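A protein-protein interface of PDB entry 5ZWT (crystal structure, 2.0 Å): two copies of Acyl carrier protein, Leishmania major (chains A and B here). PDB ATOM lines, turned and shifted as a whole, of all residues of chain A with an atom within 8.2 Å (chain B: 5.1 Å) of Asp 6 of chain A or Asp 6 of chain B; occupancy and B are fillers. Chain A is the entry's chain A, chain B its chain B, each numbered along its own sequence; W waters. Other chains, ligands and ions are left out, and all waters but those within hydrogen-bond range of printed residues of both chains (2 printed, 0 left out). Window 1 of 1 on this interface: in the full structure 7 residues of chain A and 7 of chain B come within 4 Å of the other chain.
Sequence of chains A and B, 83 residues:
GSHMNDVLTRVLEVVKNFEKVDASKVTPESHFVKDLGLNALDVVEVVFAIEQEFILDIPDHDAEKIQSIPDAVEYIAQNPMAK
The backbone NH (N) of His 3 of chain A sits close to the guanidinium group (NH1) of Arg 10 of chain B, at 3.3 Å. NH1 of Arg 10 of chain A is in salt-bridge range of OD2 of Asp 6 of chain B. The guanidinium group of Arg 10 of chain A lies close to the backbone NH of His 3 of chain B. O of Lys 83 of chain A sits close to N of His 3 of chain B. NH1 of Arg 10 of chain B lies within salt-bridge range of OD2 of Asp 6 of chain A (2.9 Å).
Ser 2 of chain A touches Arg 10 of chain B, and with the chains exchanged Arg 10 of chain A touches Ser 2 of chain B. His 3 of chain A touches Arg 10 of chain B, and with the chains exchanged Arg 10 of chain A touches His 3 of chain B. Asp 6 of chain A touches its own counterpart, Asp 6 of chain B. Asp 6 of chain A touches Arg 10 of chain B, and with the chains exchanged Arg 10 of chain A touches Asp 6 of chain B. Positions printed for both chains: 2, 3, 4, 5, 6, 7, 8, 9, 10 and 83. Of the 10 pairs that touch across the chains among the printed residues, 9 have their exchanged pair printed and touching as well.
NH2 of Arg 10 of chain B touches O of Gly 1 of chain A, 3.7 Å away. Ser 2 of chain A touches Arg 10 of chain B. His 3 of chain A touches Lys 83 of chain B. CB of Asp 6 of chain A touches OD2 of Asp 6 of chain B, at 3.7 Å. C of Ser 2 of chain B touches NH1 of Arg 10 of chain A (3.2 Å).
N of Asn 5 of chain A sits at hydrogen-bond distance from OG of Ser 2 of chain A, 3.2 Å away. O of Phe 54 of chain A lies within hydrogen-bond range of N of Lys 83 of chain A (3.2 Å). NE2 of His 3 of chain A lies within hydrogen-bond range of O of Ala 77 of chain A (3.2 Å). NH1 of Arg 10 of chain B is in hydrogen-bond range of O of Lys 83 of chain B (2.9 Å). NE of Arg 10 of chain A lies within salt-bridge range of OE1 of Glu 53 of chain A (2.7 Å). The guanidinium group (NH1) of Arg 10 of chain A sits at hydrogen-bond distance from the backbone carbonyl oxygen (O) of Lys 83 of chain A (2.5 Å).
Of the printed residues of chain B, Gly 1 of chain A touches Arg 10 (3.7 Å). Of the printed residues of chain B, His 3 of chain A touches Arg 10 (3.3 Å) and Lys 83 (3.6 Å). Printed residues of chain B within 4 Å of Arg 10 of chain A: Ser 2 (3.2 Å), His 3 (3.4 Å) and Asp 6 (3.0 Å). Ala 82 of chain A touches none of the printed residues of chain B. Printed residues of chain A within 4 Å of His 3 of chain B: Arg 10 and Lys 83. Asp 6 of chain B touches just these residues of chain A: Asp 6 (3.7 Å) and Arg 10 (3.0 Å). Printed residues of chain A within 4 Å of Lys 83 of chain B: His 3 (3.6 Å). The nearest residue of chain B that does not touch Asp 6 of chain A is Lys 83 of chain B (5.0 Å). The nearest residue of chain A that does not touch Asp 6 of chain B is Lys 83 of chain A (4.9 Å). The nearest printed residue of chain B that does not touch Lys 83 of chain A is Ser 2 of chain B (4.1 Å).
Hydrophobic or aromatic side chains of chain A that line the printed part of chain B: His 3. Among the printed residues, 10 pairs touch across the chains.
Water W1 lies within hydrogen-bond range of OD1 of Asp 6 of chain A (2.5 Å) and O of Asp 6 of chain B (2.9 Å). Water W2 lies within hydrogen-bond range of the side-chain carboxylate (OD1) of Asp 6 of chain B (2.6 Å) and the backbone carbonyl oxygen (O) of Asp 6 of chain A (2.7 Å).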
ATOM      1  N   GLY A   1     -18.429 -19.207  20.453  1.00  0.00           N
ATOM      2  CA  GLY A   1     -17.202 -19.390  19.689  1.00  0.00           C
ATOM      3  C   GLY A   1     -15.983 -18.708  20.286  1.00  0.00           C
ATOM      4  O   GLY A   1     -15.992 -18.320  21.452  1.00  0.00           O
ATOM      5  N   SER A   2     -14.933 -18.542  19.480  1.00  0.00           N
ATOM      6  CA  SER A   2     -13.701 -17.923  19.952  1.00  0.00           C
ATOM      7  C   SER A   2     -12.894 -17.458  18.753  1.00  0.00           C
ATOM      8  O   SER A   2     -13.086 -17.938  17.630  1.00  0.00           O
ATOM      9  CB  SER A   2     -12.859 -18.895  20.791  1.00  0.00           C
ATOM     10  OG  SER A   2     -12.459 -19.996  19.991  1.00  0.00           O
ATOM     11  N   HIS A   3     -11.963 -16.534  19.013  1.00  0.00           N
ATOM     12  CA  HIS A   3     -11.114 -16.019  17.938  1.00  0.00           C
ATOM     13  C   HIS A   3     -10.233 -17.107  17.346  1.00  0.00           C
ATOM     14  O   HIS A   3     -10.049 -17.171  16.122  1.00  0.00           O
ATOM     15  CB  HIS A   3     -10.239 -14.872  18.443  1.00  0.00           C
ATOM     16  CG  HIS A   3      -9.225 -14.409  17.439  1.00  0.00           C
ATOM     17  ND1 HIS A   3      -9.570 -14.007  16.166  1.00  0.00           N
ATOM     18  CD2 HIS A   3      -7.883 -14.256  17.530  1.00  0.00           C
ATOM     19  CE1 HIS A   3      -8.482 -13.645  15.510  1.00  0.00           C
ATOM     20  NE2 HIS A   3      -7.445 -13.784  16.317  1.00  0.00           N
ATOM     21  N   MET A   4      -9.681 -17.979  18.191  1.00  0.00           N
ATOM     22  CA  MET A   4      -8.817 -19.022  17.654  1.00  0.00           C
ATOM     23  C   MET A   4      -9.616 -20.001  16.802  1.00  0.00           C
ATOM     24  O   MET A   4      -9.131 -20.448  15.751  1.00  0.00           O
ATOM     25  CB  MET A   4      -8.103 -19.756  18.787  1.00  0.00           C
ATOM     26  CG  MET A   4      -7.101 -20.789  18.304  1.00  0.00           C
ATOM     27  SD  MET A   4      -6.514 -21.850  19.633  1.00  0.00           S
ATOM     28  CE  MET A   4      -7.952 -22.890  19.894  1.00  0.00           C
ATOM     29  N   ASN A   5     -10.867 -20.277  17.189  1.00  0.00           N
ATOM     30  CA  ASN A   5     -11.709 -21.151  16.376  1.00  0.00           C
ATOM     31  C   ASN A   5     -12.125 -20.483  15.078  1.00  0.00           C
ATOM     32  O   ASN A   5     -12.276 -21.169  14.064  1.00  0.00           O
ATOM     33  CB  ASN A   5     -12.955 -21.595  17.149  1.00  0.00           C
ATOM     34  CG  ASN A   5     -13.815 -22.563  16.348  1.00  0.00           C
ATOM     35  OD1 ASN A   5     -13.480 -23.741  16.228  1.00  0.00           O
ATOM     36  ND2 ASN A   5     -14.936 -22.080  15.813  1.00  0.00           N
ATOM     37  N   ASP A   6     -12.336 -19.160  15.093  1.00  0.00           N
ATOM     38  CA  ASP A   6     -12.609 -18.432  13.855  1.00  0.00           C
ATOM     39  C   ASP A   6     -11.474 -18.588  12.856  1.00  0.00           C
ATOM     40  O   ASP A   6     -11.709 -18.813  11.662  1.00  0.00           O
ATOM     41  CB  ASP A   6     -12.823 -16.947  14.138  1.00  0.00           C
ATOM     42  CG  ASP A   6     -14.108 -16.669  14.858  1.00  0.00           C
ATOM     43  OD1 ASP A   6     -15.057 -17.496  14.751  1.00  0.00           O
ATOM     44  OD2 ASP A   6     -14.157 -15.616  15.528  1.00  0.00           O
ATOM     45  N   VAL A   7     -10.233 -18.420  13.321  1.00  0.00           N
ATOM     46  CA  VAL A   7      -9.079 -18.583  12.441  1.00  0.00           C
ATOM     47  C   VAL A   7      -8.986 -20.024  11.973  1.00  0.00           C
ATOM     48  O   VAL A   7      -8.776 -20.303  10.784  1.00  0.00           O
ATOM     49  CB  VAL A   7      -7.792 -18.155  13.163  1.00  0.00           C
ATOM     50  CG1 VAL A   7      -6.561 -18.502  12.314  1.00  0.00           C
ATOM     51  CG2 VAL A   7      -7.836 -16.671  13.477  1.00  0.00           C
ATOM     52  N   LEU A   8      -9.147 -20.960  12.912  1.00  0.00           N
ATOM     53  CA  LEU A   8      -9.027 -22.376  12.580  1.00  0.00           C
ATOM     54  C   LEU A   8     -10.036 -22.770  11.515  1.00  0.00           C
ATOM     55  O   LEU A   8      -9.694 -23.465  10.559  1.00  0.00           O
ATOM     56  CB  LEU A   8      -9.242 -23.213  13.845  1.00  0.00           C
ATOM     57  CG  LEU A   8      -9.367 -24.728  13.668  1.00  0.00           C
ATOM     58  CD1 LEU A   8      -8.166 -25.337  12.934  1.00  0.00           C
ATOM     59  CD2 LEU A   8      -9.602 -25.417  15.023  1.00  0.00           C
ATOM     60  N   THR A   9     -11.279 -22.303  11.658  1.00  0.00           N
ATOM     61  CA  THR A   9     -12.334 -22.616  10.695  1.00  0.00           C
ATOM     62  C   THR A   9     -11.947 -22.163   9.297  1.00  0.00           C
ATOM     63  O   THR A   9     -12.185 -22.869   8.296  1.00  0.00           O
ATOM     64  CB  THR A   9     -13.639 -21.938  11.125  1.00  0.00           C
ATOM     65  OG1 THR A   9     -14.048 -22.415  12.420  1.00  0.00           O
ATOM     66  CG2 THR A   9     -14.742 -22.190  10.113  1.00  0.00           C
ATOM     67  N   ARG A  10     -11.347 -20.983   9.198  1.00  0.00           N
ATOM     68  CA  ARG A  10     -11.000 -20.528   7.864  1.00  0.00           C
ATOM     69  C   ARG A  10      -9.731 -21.206   7.360  1.00  0.00           C
ATOM     70  O   ARG A  10      -9.631 -21.483   6.166  1.00  0.00           O
ATOM     71  CB  ARG A  10     -10.889 -19.005   7.855  1.00  0.00           C
ATOM     72  CG  ARG A  10     -12.246 -18.317   8.122  1.00  0.00           C
ATOM     73  CD  ARG A  10     -12.065 -16.857   8.481  1.00  0.00           C
ATOM     74  NE  ARG A  10     -11.300 -16.129   7.479  1.00  0.00           N
ATOM     75  CZ  ARG A  10     -10.868 -14.880   7.651  1.00  0.00           C
ATOM     76  NH1 ARG A  10     -11.140 -14.240   8.780  1.00  0.00           N
ATOM     77  NH2 ARG A  10     -10.167 -14.270   6.700  1.00  0.00           N
ATOM     78  N   VAL A  11      -8.786 -21.543   8.243  1.00  0.00           N
ATOM     79  CA  VAL A  11      -7.620 -22.285   7.756  1.00  0.00           C
ATOM     80  C   VAL A  11      -8.032 -23.664   7.263  1.00  0.00           C
ATOM     81  O   VAL A  11      -7.541 -24.138   6.226  1.00  0.00           O
ATOM     82  CB  VAL A  11      -6.522 -22.382   8.832  1.00  0.00           C
ATOM     83  CG1 VAL A  11      -5.400 -23.331   8.353  1.00  0.00           C
ATOM     84  CG2 VAL A  11      -5.952 -21.008   9.102  1.00  0.00           C
ATOM     85  N   LEU A  12      -8.970 -24.312   7.965  1.00  0.00           N
ATOM     86  CA  LEU A  12      -9.378 -25.661   7.572  1.00  0.00           C
ATOM     87  C   LEU A  12      -9.958 -25.649   6.175  1.00  0.00           C
ATOM     88  O   LEU A  12      -9.686 -26.557   5.382  1.00  0.00           O
ATOM     89  CB  LEU A  12     -10.398 -26.247   8.560  1.00  0.00           C
ATOM     90  CG  LEU A  12      -9.903 -26.692   9.945  1.00  0.00           C
ATOM     91  CD1 LEU A  12     -11.081 -27.003  10.840  1.00  0.00           C
ATOM     92  CD2 LEU A  12      -8.987 -27.899   9.837  1.00  0.00           C
ATOM     93  N   GLU A  53      -6.298 -15.641   2.190  1.00  0.00           N
ATOM     94  CA  GLU A  53      -7.521 -15.757   2.967  1.00  0.00           C
ATOM     95  C   GLU A  53      -7.567 -14.699   4.061  1.00  0.00           C
ATOM     96  O   GLU A  53      -8.614 -14.085   4.297  1.00  0.00           O
ATOM     97  CB  GLU A  53      -7.632 -17.164   3.568  1.00  0.00           C
ATOM     98  CG  GLU A  53      -8.714 -17.303   4.639  1.00  0.00           C
ATOM     99  CD  GLU A  53     -10.129 -17.104   4.084  1.00  0.00           C
ATOM    100  OE1 GLU A  53     -11.035 -16.813   4.887  1.00  0.00           O
ATOM    101  OE2 GLU A  53     -10.348 -17.226   2.856  1.00  0.00           O
ATOM    102  N   PHE A  54      -6.432 -14.419   4.689  1.00  0.00           N
ATOM    103  CA  PHE A  54      -6.392 -13.486   5.804  1.00  0.00           C
ATOM    104  C   PHE A  54      -5.785 -12.142   5.422  1.00  0.00           C
ATOM    105  O   PHE A  54      -5.568 -11.308   6.304  1.00  0.00           O
ATOM    106  CB  PHE A  54      -5.629 -14.102   6.983  1.00  0.00           C
ATOM    107  CG  PHE A  54      -6.328 -15.292   7.604  1.00  0.00           C
ATOM    108  CD1 PHE A  54      -7.299 -15.117   8.590  1.00  0.00           C
ATOM    109  CD2 PHE A  54      -6.033 -16.577   7.178  1.00  0.00           C
ATOM    110  CE1 PHE A  54      -7.950 -16.214   9.146  1.00  0.00           C
ATOM    111  CE2 PHE A  54      -6.679 -17.678   7.728  1.00  0.00           C
ATOM    112  CZ  PHE A  54      -7.633 -17.494   8.719  1.00  0.00           C
ATOM    113  N   VAL A  73      -2.544 -21.719  12.487  1.00  0.00           N
ATOM    114  CA  VAL A  73      -3.551 -21.089  13.331  1.00  0.00           C
ATOM    115  C   VAL A  73      -2.896 -20.298  14.461  1.00  0.00           C
ATOM    116  O   VAL A  73      -3.313 -19.174  14.766  1.00  0.00           O
ATOM    117  CB  VAL A  73      -4.537 -22.147  13.856  1.00  0.00           C
ATOM    118  CG1 VAL A  73      -5.468 -21.533  14.872  1.00  0.00           C
ATOM    119  CG2 VAL A  73      -5.352 -22.714  12.688  1.00  0.00           C
ATOM    120  N   ILE A  76      -1.477 -17.068  12.774  1.00  0.00           N
ATOM    121  CA  ILE A  76      -2.470 -16.121  12.281  1.00  0.00           C
ATOM    122  C   ILE A  76      -3.233 -15.497  13.442  1.00  0.00           C
ATOM    123  O   ILE A  76      -3.467 -14.282  13.467  1.00  0.00           O
ATOM    124  CB  ILE A  76      -3.424 -16.804  11.282  1.00  0.00           C
ATOM    125  CG1 ILE A  76      -2.669 -17.292  10.038  1.00  0.00           C
ATOM    126  CG2 ILE A  76      -4.537 -15.836  10.867  1.00  0.00           C
ATOM    127  CD1 ILE A  76      -2.148 -16.187   9.164  1.00  0.00           C
ATOM    128  N   ALA A  77      -3.616 -16.308  14.429  1.00  0.00           N
ATOM    129  CA  ALA A  77      -4.404 -15.789  15.541  1.00  0.00           C
ATOM    130  C   ALA A  77      -3.642 -14.730  16.333  1.00  0.00           C
ATOM    131  O   ALA A  77      -4.253 -13.786  16.850  1.00  0.00           O
ATOM    132  CB  ALA A  77      -4.831 -16.933  16.460  1.00  0.00           C
ATOM    133  N   ALA A  82      -4.957  -8.765  10.367  1.00  0.00           N
ATOM    134  CA  ALA A  82      -5.757  -9.944  10.058  1.00  0.00           C
ATOM    135  C   ALA A  82      -7.046  -9.501   9.393  1.00  0.00           C
ATOM    136  O   ALA A  82      -7.498  -8.366   9.564  1.00  0.00           O
ATOM    137  CB  ALA A  82      -6.066 -10.770  11.311  1.00  0.00           C
ATOM    138  N   LYS A  83      -7.624 -10.408   8.621  1.00  0.00           N
ATOM    139  CA  LYS A  83      -8.910 -10.145   7.998  1.00  0.00           C
ATOM    140  C   LYS A  83      -9.716 -11.428   7.929  1.00  0.00           C
ATOM    141  O   LYS A  83      -9.547 -12.308   8.767  1.00  0.00           O
ATOM    142  CB  LYS A  83      -8.727  -9.541   6.609  1.00  0.00           C
ATOM    143  N   SER B   2     -14.075 -13.870   6.434  1.00  0.00           N
ATOM    144  CA  SER B   2     -13.526 -12.562   6.787  1.00  0.00           C
ATOM    145  C   SER B   2     -13.677 -12.337   8.285  1.00  0.00           C
ATOM    146  O   SER B   2     -14.455 -13.018   8.955  1.00  0.00           O
ATOM    147  CB  SER B   2     -14.216 -11.437   6.011  1.00  0.00           C
ATOM    148  OG  SER B   2     -15.592 -11.392   6.324  1.00  0.00           O
ATOM    149  N   HIS B   3     -12.899 -11.389   8.814  1.00  0.00           N
ATOM    150  CA  HIS B   3     -13.018 -11.071  10.237  1.00  0.00           C
ATOM    151  C   HIS B   3     -14.394 -10.496  10.548  1.00  0.00           C
ATOM    152  O   HIS B   3     -14.964 -10.759  11.615  1.00  0.00           O
ATOM    153  CB  HIS B   3     -11.912 -10.106  10.672  1.00  0.00           C
ATOM    154  CG  HIS B   3     -12.032  -9.650  12.096  1.00  0.00           C
ATOM    155  ND1 HIS B   3     -12.075 -10.529  13.158  1.00  0.00           N
ATOM    156  CD2 HIS B   3     -12.122  -8.408  12.633  1.00  0.00           C
ATOM    157  CE1 HIS B   3     -12.184  -9.849  14.286  1.00  0.00           C
ATOM    158  NE2 HIS B   3     -12.211  -8.560  13.997  1.00  0.00           N
ATOM    159  N   MET B   4     -14.943  -9.695   9.631  1.00  0.00           N
ATOM    160  CA  MET B   4     -16.255  -9.115   9.877  1.00  0.00           C
ATOM    161  C   MET B   4     -17.330 -10.194   9.876  1.00  0.00           C
ATOM    162  O   MET B   4     -18.266 -10.147  10.684  1.00  0.00           O
ATOM    163  CB  MET B   4     -16.549  -8.041   8.824  1.00  0.00           C
ATOM    164  CG  MET B   4     -17.865  -7.272   8.975  1.00  0.00           C
ATOM    165  SD  MET B   4     -17.759  -5.950  10.197  1.00  0.00           S
ATOM    166  CE  MET B   4     -16.245  -5.137   9.685  1.00  0.00           C
ATOM    167  N   ASN B   5     -17.203 -11.195   9.005  1.00  0.00           N
ATOM    168  CA  ASN B   5     -18.178 -12.278   9.051  1.00  0.00           C
ATOM    169  C   ASN B   5     -17.980 -13.146  10.281  1.00  0.00           C
ATOM    170  O   ASN B   5     -18.965 -13.613  10.863  1.00  0.00           O
ATOM    171  CB  ASN B   5     -18.128 -13.113   7.774  1.00  0.00           C
ATOM    172  CG  ASN B   5     -19.136 -14.251   7.792  1.00  0.00           C
ATOM    173  OD1 ASN B   5     -20.338 -14.035   7.627  1.00  0.00           O
ATOM    174  ND2 ASN B   5     -18.641 -15.481   7.937  1.00  0.00           N
ATOM    175  N   ASP B   6     -16.729 -13.331  10.712  1.00  0.00           N
ATOM    176  CA  ASP B   6     -16.480 -14.058  11.951  1.00  0.00           C
ATOM    177  C   ASP B   6     -17.193 -13.389  13.116  1.00  0.00           C
ATOM    178  O   ASP B   6     -17.854 -14.060  13.920  1.00  0.00           O
ATOM    179  CB  ASP B   6     -14.978 -14.131  12.237  1.00  0.00           C
ATOM    180  CG  ASP B   6     -14.219 -14.998  11.239  1.00  0.00           C
ATOM    181  OD1 ASP B   6     -14.859 -15.863  10.598  1.00  0.00           O
ATOM    182  OD2 ASP B   6     -12.972 -14.840  11.143  1.00  0.00           O
ATOM    183  N   VAL B   7     -17.096 -12.061  13.201  1.00  0.00           N
ATOM    184  CA  VAL B   7     -17.746 -11.325  14.283  1.00  0.00           C
ATOM    185  C   VAL B   7     -19.259 -11.445  14.184  1.00  0.00           C
ATOM    186  O   VAL B   7     -19.931 -11.779  15.169  1.00  0.00           O
ATOM    187  CB  VAL B   7     -17.289  -9.857  14.265  1.00  0.00           C
ATOM    188  CG1 VAL B   7     -18.142  -9.028  15.229  1.00  0.00           C
ATOM    189  CG2 VAL B   7     -15.825  -9.784  14.680  1.00  0.00           C
ATOM    190  N   LEU B   8     -19.806 -11.234  12.982  1.00  0.00           N
ATOM    191  CA  LEU B   8     -21.250 -11.283  12.780  1.00  0.00           C
ATOM    192  C   LEU B   8     -21.816 -12.644  13.136  1.00  0.00           C
ATOM    193  O   LEU B   8     -22.920 -12.737  13.690  1.00  0.00           O
ATOM    194  CB  LEU B   8     -21.578 -10.917  11.330  1.00  0.00           C
ATOM    195  CG  LEU B   8     -22.989 -10.943  10.735  1.00  0.00           C
ATOM    196  CD1 LEU B   8     -23.281 -12.298  10.121  1.00  0.00           C
ATOM    197  CD2 LEU B   8     -24.076 -10.553  11.734  1.00  0.00           C
ATOM    198  N   THR B   9     -21.095 -13.712  12.779  1.00  0.00           N
ATOM    199  CA  THR B   9     -21.581 -15.061  13.051  1.00  0.00           C
ATOM    200  C   THR B   9     -21.778 -15.267  14.544  1.00  0.00           C
ATOM    201  O   THR B   9     -22.790 -15.832  14.971  1.00  0.00           O
ATOM    202  CB  THR B   9     -20.609 -16.099  12.477  1.00  0.00           C
ATOM    203  OG1 THR B   9     -20.482 -15.906  11.058  1.00  0.00           O
ATOM    204  CG2 THR B   9     -21.132 -17.518  12.703  1.00  0.00           C
ATOM    205  N   ARG B  10     -20.841 -14.772  15.358  1.00  0.00           N
ATOM    206  CA  ARG B  10     -20.935 -14.969  16.803  1.00  0.00           C
ATOM    207  C   ARG B  10     -21.917 -14.019  17.468  1.00  0.00           C
ATOM    208  O   ARG B  10     -22.579 -14.419  18.432  1.00  0.00           O
ATOM    209  CB  ARG B  10     -19.554 -14.838  17.441  1.00  0.00           C
ATOM    210  CG  ARG B  10     -18.628 -15.960  16.978  1.00  0.00           C
ATOM    211  CD  ARG B  10     -17.172 -15.695  17.276  1.00  0.00           C
ATOM    212  NE  ARG B  10     -16.915 -15.409  18.685  1.00  0.00           N
ATOM    213  CZ  ARG B  10     -15.733 -15.025  19.146  1.00  0.00           C
ATOM    214  NH1 ARG B  10     -14.716 -14.907  18.305  1.00  0.00           N
ATOM    215  NH2 ARG B  10     -15.563 -14.766  20.439  1.00  0.00           N
ATOM    216  N   LYS B  83     -11.695 -10.897  21.174  1.00  0.00           N
ATOM    217  CA  LYS B  83     -11.301 -12.300  21.147  1.00  0.00           C
ATOM    218  C   LYS B  83     -12.503 -13.171  20.813  1.00  0.00           C
ATOM    219  O   LYS B  83     -13.058 -13.064  19.720  1.00  0.00           O
ATOM    220  CB  LYS B  83     -10.699 -12.718  22.490  1.00  0.00           C
HETATM  221  O   HOH W   1     -17.295 -16.855  13.915  1.00  0.00           O
HETATM  222  O   HOH W   2     -14.238 -18.355  10.759  1.00  0.00           O
